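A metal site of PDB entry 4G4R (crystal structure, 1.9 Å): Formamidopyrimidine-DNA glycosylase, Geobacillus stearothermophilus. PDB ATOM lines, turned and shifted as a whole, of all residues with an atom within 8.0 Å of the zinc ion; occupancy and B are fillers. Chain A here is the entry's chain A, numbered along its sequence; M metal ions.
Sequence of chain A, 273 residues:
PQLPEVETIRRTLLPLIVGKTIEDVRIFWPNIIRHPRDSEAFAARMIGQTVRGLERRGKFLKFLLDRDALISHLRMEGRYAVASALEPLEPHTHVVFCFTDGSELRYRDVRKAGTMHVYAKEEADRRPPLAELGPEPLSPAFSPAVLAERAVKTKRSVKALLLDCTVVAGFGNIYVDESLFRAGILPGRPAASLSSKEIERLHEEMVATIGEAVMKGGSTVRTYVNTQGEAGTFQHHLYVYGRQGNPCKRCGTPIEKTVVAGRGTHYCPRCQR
The side-chain sulfur (SG) of Cys 268 lies close to the backbone NH (N) of Arg 270 (3.4 Å).
The side-chain amide oxygen of Gln 272 sits at hydrogen-bond distance from the backbone NH of Cys 268 (2.8 Å).
N of Arg 250 lies close to SG of Cys 248 (3.4 Å).
The backbone carbonyl oxygen of Thr 253 lies within hydrogen-bond range of the backbone NH of Cys 248 (2.7 Å).
The side-chain sulfur (SG) of Cys 251 lies close to the side-chain hydroxyl (OG1) of Thr 253, at 3.1 Å.
Four residues have an atom within 4 Å of the zinc ion: Cys 248, Cys 251, Cys 268 and Cys 271.
The side-chain sulfur (SG) of Cys 268 binds the zinc ion, at 2.3 Å.
SG of Cys 248 binds the zinc ion, 2.3 Å away.
The side-chain sulfur (SG) of Cys 251 binds the zinc ion, at 2.3 Å.
The zinc ion is bound by SG of Cys 271 (2.3 Å).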
ATOM      1  N   PHE A 181     -31.401 -12.681  -0.994  1.00  0.00           N
ATOM      2  CA  PHE A 181     -30.305 -12.754  -0.038  1.00  0.00           C
ATOM      3  C   PHE A 181     -30.418 -13.992   0.846  1.00  0.00           C
ATOM      4  O   PHE A 181     -29.468 -14.747   1.023  1.00  0.00           O
ATOM      5  CB  PHE A 181     -30.244 -11.517   0.873  1.00  0.00           C
ATOM      6  CG  PHE A 181     -29.276 -11.700   2.012  1.00  0.00           C
ATOM      7  CD1 PHE A 181     -27.924 -11.518   1.823  1.00  0.00           C
ATOM      8  CD2 PHE A 181     -29.726 -12.129   3.274  1.00  0.00           C
ATOM      9  CE1 PHE A 181     -27.010 -11.705   2.852  1.00  0.00           C
ATOM     10  CE2 PHE A 181     -28.813 -12.312   4.312  1.00  0.00           C
ATOM     11  CZ  PHE A 181     -27.460 -12.113   4.106  1.00  0.00           C
ATOM     12  N   TYR A 239     -31.841  -7.487   5.780  1.00  0.00           N
ATOM     13  CA  TYR A 239     -30.487  -7.951   5.521  1.00  0.00           C
ATOM     14  C   TYR A 239     -29.749  -7.091   4.512  1.00  0.00           C
ATOM     15  O   TYR A 239     -28.554  -6.827   4.677  1.00  0.00           O
ATOM     16  CB  TYR A 239     -30.510  -9.401   5.052  1.00  0.00           C
ATOM     17  CG  TYR A 239     -30.810 -10.387   6.156  1.00  0.00           C
ATOM     18  CD1 TYR A 239     -32.059 -10.989   6.259  1.00  0.00           C
ATOM     19  CD2 TYR A 239     -29.839 -10.712   7.104  1.00  0.00           C
ATOM     20  CE1 TYR A 239     -32.330 -11.892   7.268  1.00  0.00           C
ATOM     21  CE2 TYR A 239     -30.106 -11.624   8.117  1.00  0.00           C
ATOM     22  CZ  TYR A 239     -31.353 -12.212   8.193  1.00  0.00           C
ATOM     23  OH  TYR A 239     -31.625 -13.116   9.203  1.00  0.00           O
ATOM     24  N   VAL A 240     -30.445  -6.666   3.461  1.00  0.00           N
ATOM     25  CA  VAL A 240     -29.751  -5.987   2.369  1.00  0.00           C
ATOM     26  C   VAL A 240     -30.443  -4.726   1.875  1.00  0.00           C
ATOM     27  O   VAL A 240     -29.758  -3.775   1.504  1.00  0.00           O
ATOM     28  CB  VAL A 240     -29.493  -6.937   1.146  1.00  0.00           C
ATOM     29  CG1 VAL A 240     -28.543  -8.069   1.514  1.00  0.00           C
ATOM     30  CG2 VAL A 240     -30.801  -7.499   0.572  1.00  0.00           C
ATOM     31  N   PRO A 247     -22.164  -3.355   6.546  1.00  0.00           N
ATOM     32  CA  PRO A 247     -21.735  -4.761   6.635  1.00  0.00           C
ATOM     33  C   PRO A 247     -22.913  -5.733   6.576  1.00  0.00           C
ATOM     34  O   PRO A 247     -23.963  -5.522   7.195  1.00  0.00           O
ATOM     35  CB  PRO A 247     -21.060  -4.838   8.011  1.00  0.00           C
ATOM     36  CG  PRO A 247     -20.723  -3.418   8.366  1.00  0.00           C
ATOM     37  CD  PRO A 247     -21.822  -2.588   7.760  1.00  0.00           C
ATOM     38  N   CYS A 248     -22.736  -6.788   5.796  1.00  0.00           N
ATOM     39  CA  CYS A 248     -23.681  -7.889   5.773  1.00  0.00           C
ATOM     40  C   CYS A 248     -23.809  -8.417   7.197  1.00  0.00           C
ATOM     41  O   CYS A 248     -22.823  -8.575   7.897  1.00  0.00           O
ATOM     42  CB  CYS A 248     -23.186  -8.991   4.833  1.00  0.00           C
ATOM     43  SG  CYS A 248     -24.217 -10.462   4.841  1.00  0.00           S
ATOM     44  N   LYS A 249     -25.038  -8.690   7.614  1.00  0.00           N
ATOM     45  CA  LYS A 249     -25.310  -9.168   8.964  1.00  0.00           C
ATOM     46  C   LYS A 249     -24.897 -10.612   9.152  1.00  0.00           C
ATOM     47  O   LYS A 249     -24.803 -11.090  10.282  1.00  0.00           O
ATOM     48  CB  LYS A 249     -26.799  -8.984   9.300  1.00  0.00           C
ATOM     49  CG  LYS A 249     -27.225  -7.520   9.286  1.00  0.00           C
ATOM     50  CD  LYS A 249     -28.696  -7.342   9.669  1.00  0.00           C
ATOM     51  CE  LYS A 249     -29.068  -5.863   9.707  1.00  0.00           C
ATOM     52  NZ  LYS A 249     -30.475  -5.621  10.135  1.00  0.00           N
ATOM     53  N   ARG A 250     -24.661 -11.328   8.050  1.00  0.00           N
ATOM     54  CA  ARG A 250     -24.232 -12.734   8.139  1.00  0.00           C
ATOM     55  C   ARG A 250     -22.717 -12.937   7.952  1.00  0.00           C
ATOM     56  O   ARG A 250     -22.129 -13.842   8.557  1.00  0.00           O
ATOM     57  CB  ARG A 250     -24.990 -13.570   7.102  1.00  0.00           C
ATOM     58  CG  ARG A 250     -26.477 -13.699   7.410  1.00  0.00           C
ATOM     59  CD  ARG A 250     -26.811 -15.095   7.918  1.00  0.00           C
ATOM     60  NE  ARG A 250     -28.227 -15.281   8.232  1.00  0.00           N
ATOM     61  CZ  ARG A 250     -29.150 -15.624   7.334  1.00  0.00           C
ATOM     62  NH1 ARG A 250     -28.825 -15.797   6.061  1.00  0.00           N
ATOM     63  NH2 ARG A 250     -30.418 -15.777   7.712  1.00  0.00           N
ATOM     64  N   CYS A 251     -22.081 -12.128   7.117  1.00  0.00           N
ATOM     65  CA  CYS A 251     -20.670 -12.369   6.829  1.00  0.00           C
ATOM     66  C   CYS A 251     -19.787 -11.119   6.939  1.00  0.00           C
ATOM     67  O   CYS A 251     -18.562 -11.223   6.884  1.00  0.00           O
ATOM     68  CB  CYS A 251     -20.521 -12.970   5.428  1.00  0.00           C
ATOM     69  SG  CYS A 251     -20.715 -11.724   4.097  1.00  0.00           S
ATOM     70  N   GLY A 252     -20.403  -9.947   7.067  1.00  0.00           N
ATOM     71  CA  GLY A 252     -19.667  -8.717   7.280  1.00  0.00           C
ATOM     72  C   GLY A 252     -19.168  -8.018   6.024  1.00  0.00           C
ATOM     73  O   GLY A 252     -18.603  -6.927   6.096  1.00  0.00           O
ATOM     74  N   THR A 253     -19.369  -8.645   4.875  1.00  0.00           N
ATOM     75  CA  THR A 253     -19.015  -8.042   3.602  1.00  0.00           C
ATOM     76  C   THR A 253     -19.934  -6.837   3.338  1.00  0.00           C
ATOM     77  O   THR A 253     -21.132  -6.902   3.611  1.00  0.00           O
ATOM     78  CB  THR A 253     -19.193  -9.062   2.469  1.00  0.00           C
ATOM     79  OG1 THR A 253     -18.402 -10.229   2.751  1.00  0.00           O
ATOM     80  CG2 THR A 253     -18.797  -8.470   1.117  1.00  0.00           C
ATOM     81  N   PRO A 254     -19.371  -5.731   2.832  1.00  0.00           N
ATOM     82  CA  PRO A 254     -20.268  -4.592   2.585  1.00  0.00           C
ATOM     83  C   PRO A 254     -21.358  -4.916   1.569  1.00  0.00           C
ATOM     84  O   PRO A 254     -21.092  -5.494   0.524  1.00  0.00           O
ATOM     85  CB  PRO A 254     -19.335  -3.497   2.049  1.00  0.00           C
ATOM     86  CG  PRO A 254     -17.951  -3.879   2.643  1.00  0.00           C
ATOM     87  CD  PRO A 254     -17.952  -5.391   2.619  1.00  0.00           C
ATOM     88  N   ILE A 255     -22.594  -4.521   1.886  1.00  0.00           N
ATOM     89  CA  ILE A 255     -23.697  -4.686   0.947  1.00  0.00           C
ATOM     90  C   ILE A 255     -23.506  -3.774  -0.255  1.00  0.00           C
ATOM     91  O   ILE A 255     -23.112  -2.616  -0.127  1.00  0.00           O
ATOM     92  CB  ILE A 255     -25.049  -4.431   1.643  1.00  0.00           C
ATOM     93  CG1 ILE A 255     -25.212  -5.437   2.787  1.00  0.00           C
ATOM     94  CG2 ILE A 255     -26.216  -4.565   0.655  1.00  0.00           C
ATOM     95  CD1 ILE A 255     -24.994  -6.874   2.333  1.00  0.00           C
ATOM     96  N   TYR A 267     -27.572  -6.436  -2.492  1.00  0.00           N
ATOM     97  CA  TYR A 267     -27.145  -7.825  -2.335  1.00  0.00           C
ATOM     98  C   TYR A 267     -25.787  -7.918  -1.629  1.00  0.00           C
ATOM     99  O   TYR A 267     -25.013  -6.945  -1.581  1.00  0.00           O
ATOM    100  CB  TYR A 267     -27.091  -8.523  -3.705  1.00  0.00           C
ATOM    101  CG  TYR A 267     -26.072  -7.903  -4.630  1.00  0.00           C
ATOM    102  CD1 TYR A 267     -24.776  -8.414  -4.703  1.00  0.00           C
ATOM    103  CD2 TYR A 267     -26.376  -6.765  -5.378  1.00  0.00           C
ATOM    104  CE1 TYR A 267     -23.819  -7.829  -5.522  1.00  0.00           C
ATOM    105  CE2 TYR A 267     -25.414  -6.167  -6.202  1.00  0.00           C
ATOM    106  CZ  TYR A 267     -24.136  -6.708  -6.265  1.00  0.00           C
ATOM    107  OH  TYR A 267     -23.166  -6.144  -7.065  1.00  0.00           O
ATOM    108  N   CYS A 268     -25.509  -9.096  -1.082  1.00  0.00           N
ATOM    109  CA  CYS A 268     -24.180  -9.378  -0.554  1.00  0.00           C
ATOM    110  C   CYS A 268     -23.436 -10.226  -1.573  1.00  0.00           C
ATOM    111  O   CYS A 268     -23.915 -11.312  -1.962  1.00  0.00           O
ATOM    112  CB  CYS A 268     -24.255 -10.106   0.791  1.00  0.00           C
ATOM    113  SG  CYS A 268     -22.631 -10.614   1.389  1.00  0.00           S
ATOM    114  N   PRO A 269     -22.288  -9.728  -2.041  1.00  0.00           N
ATOM    115  CA  PRO A 269     -21.601 -10.469  -3.107  1.00  0.00           C
ATOM    116  C   PRO A 269     -20.881 -11.711  -2.575  1.00  0.00           C
ATOM    117  O   PRO A 269     -20.349 -12.484  -3.360  1.00  0.00           O
ATOM    118  CB  PRO A 269     -20.591  -9.442  -3.642  1.00  0.00           C
ATOM    119  CG  PRO A 269     -20.303  -8.549  -2.461  1.00  0.00           C
ATOM    120  CD  PRO A 269     -21.629  -8.451  -1.712  1.00  0.00           C
ATOM    121  N   ARG A 270     -20.851 -11.896  -1.251  1.00  0.00           N
ATOM    122  CA  ARG A 270     -20.309 -13.127  -0.673  1.00  0.00           C
ATOM    123  C   ARG A 270     -21.372 -14.188  -0.376  1.00  0.00           C
ATOM    124  O   ARG A 270     -21.202 -15.341  -0.730  1.00  0.00           O
ATOM    125  CB  ARG A 270     -19.515 -12.846   0.605  1.00  0.00           C
ATOM    126  CG  ARG A 270     -18.898 -14.114   1.204  1.00  0.00           C
ATOM    127  CD  ARG A 270     -18.034 -13.829   2.432  1.00  0.00           C
ATOM    128  NE  ARG A 270     -17.450 -15.076   2.923  1.00  0.00           N
ATOM    129  CZ  ARG A 270     -16.590 -15.156   3.928  1.00  0.00           C
ATOM    130  NH1 ARG A 270     -16.094 -16.344   4.270  1.00  0.00           N
ATOM    131  NH2 ARG A 270     -16.212 -14.056   4.583  1.00  0.00           N
ATOM    132  N   CYS A 271     -22.451 -13.787   0.296  1.00  0.00           N
ATOM    133  CA  CYS A 271     -23.520 -14.736   0.635  1.00  0.00           C
ATOM    134  C   CYS A 271     -24.321 -15.193  -0.565  1.00  0.00           C
ATOM    135  O   CYS A 271     -24.841 -16.315  -0.566  1.00  0.00           O
ATOM    136  CB  CYS A 271     -24.486 -14.159   1.688  1.00  0.00           C
ATOM    137  SG  CYS A 271     -23.738 -13.940   3.299  1.00  0.00           S
ATOM    138  N   GLN A 272     -24.434 -14.349  -1.581  1.00  0.00           N
ATOM    139  CA  GLN A 272     -25.244 -14.664  -2.751  1.00  0.00           C
ATOM    140  C   GLN A 272     -24.379 -15.057  -3.927  1.00  0.00           C
ATOM    141  O   GLN A 272     -23.365 -14.420  -4.192  1.00  0.00           O
ATOM    142  CB  GLN A 272     -26.141 -13.479  -3.113  1.00  0.00           C
ATOM    143  CG  GLN A 272     -27.140 -13.168  -1.991  1.00  0.00           C
ATOM    144  CD  GLN A 272     -27.882 -11.849  -2.178  1.00  0.00           C
ATOM    145  OE1 GLN A 272     -27.624 -10.898  -1.442  1.00  0.00           O
ATOM    146  NE2 GLN A 272     -28.837 -11.810  -3.109  1.00  0.00           N
HETATM  147 ZN    ZN M   1     -22.936 -11.741   3.376  1.00  0.00          ZN
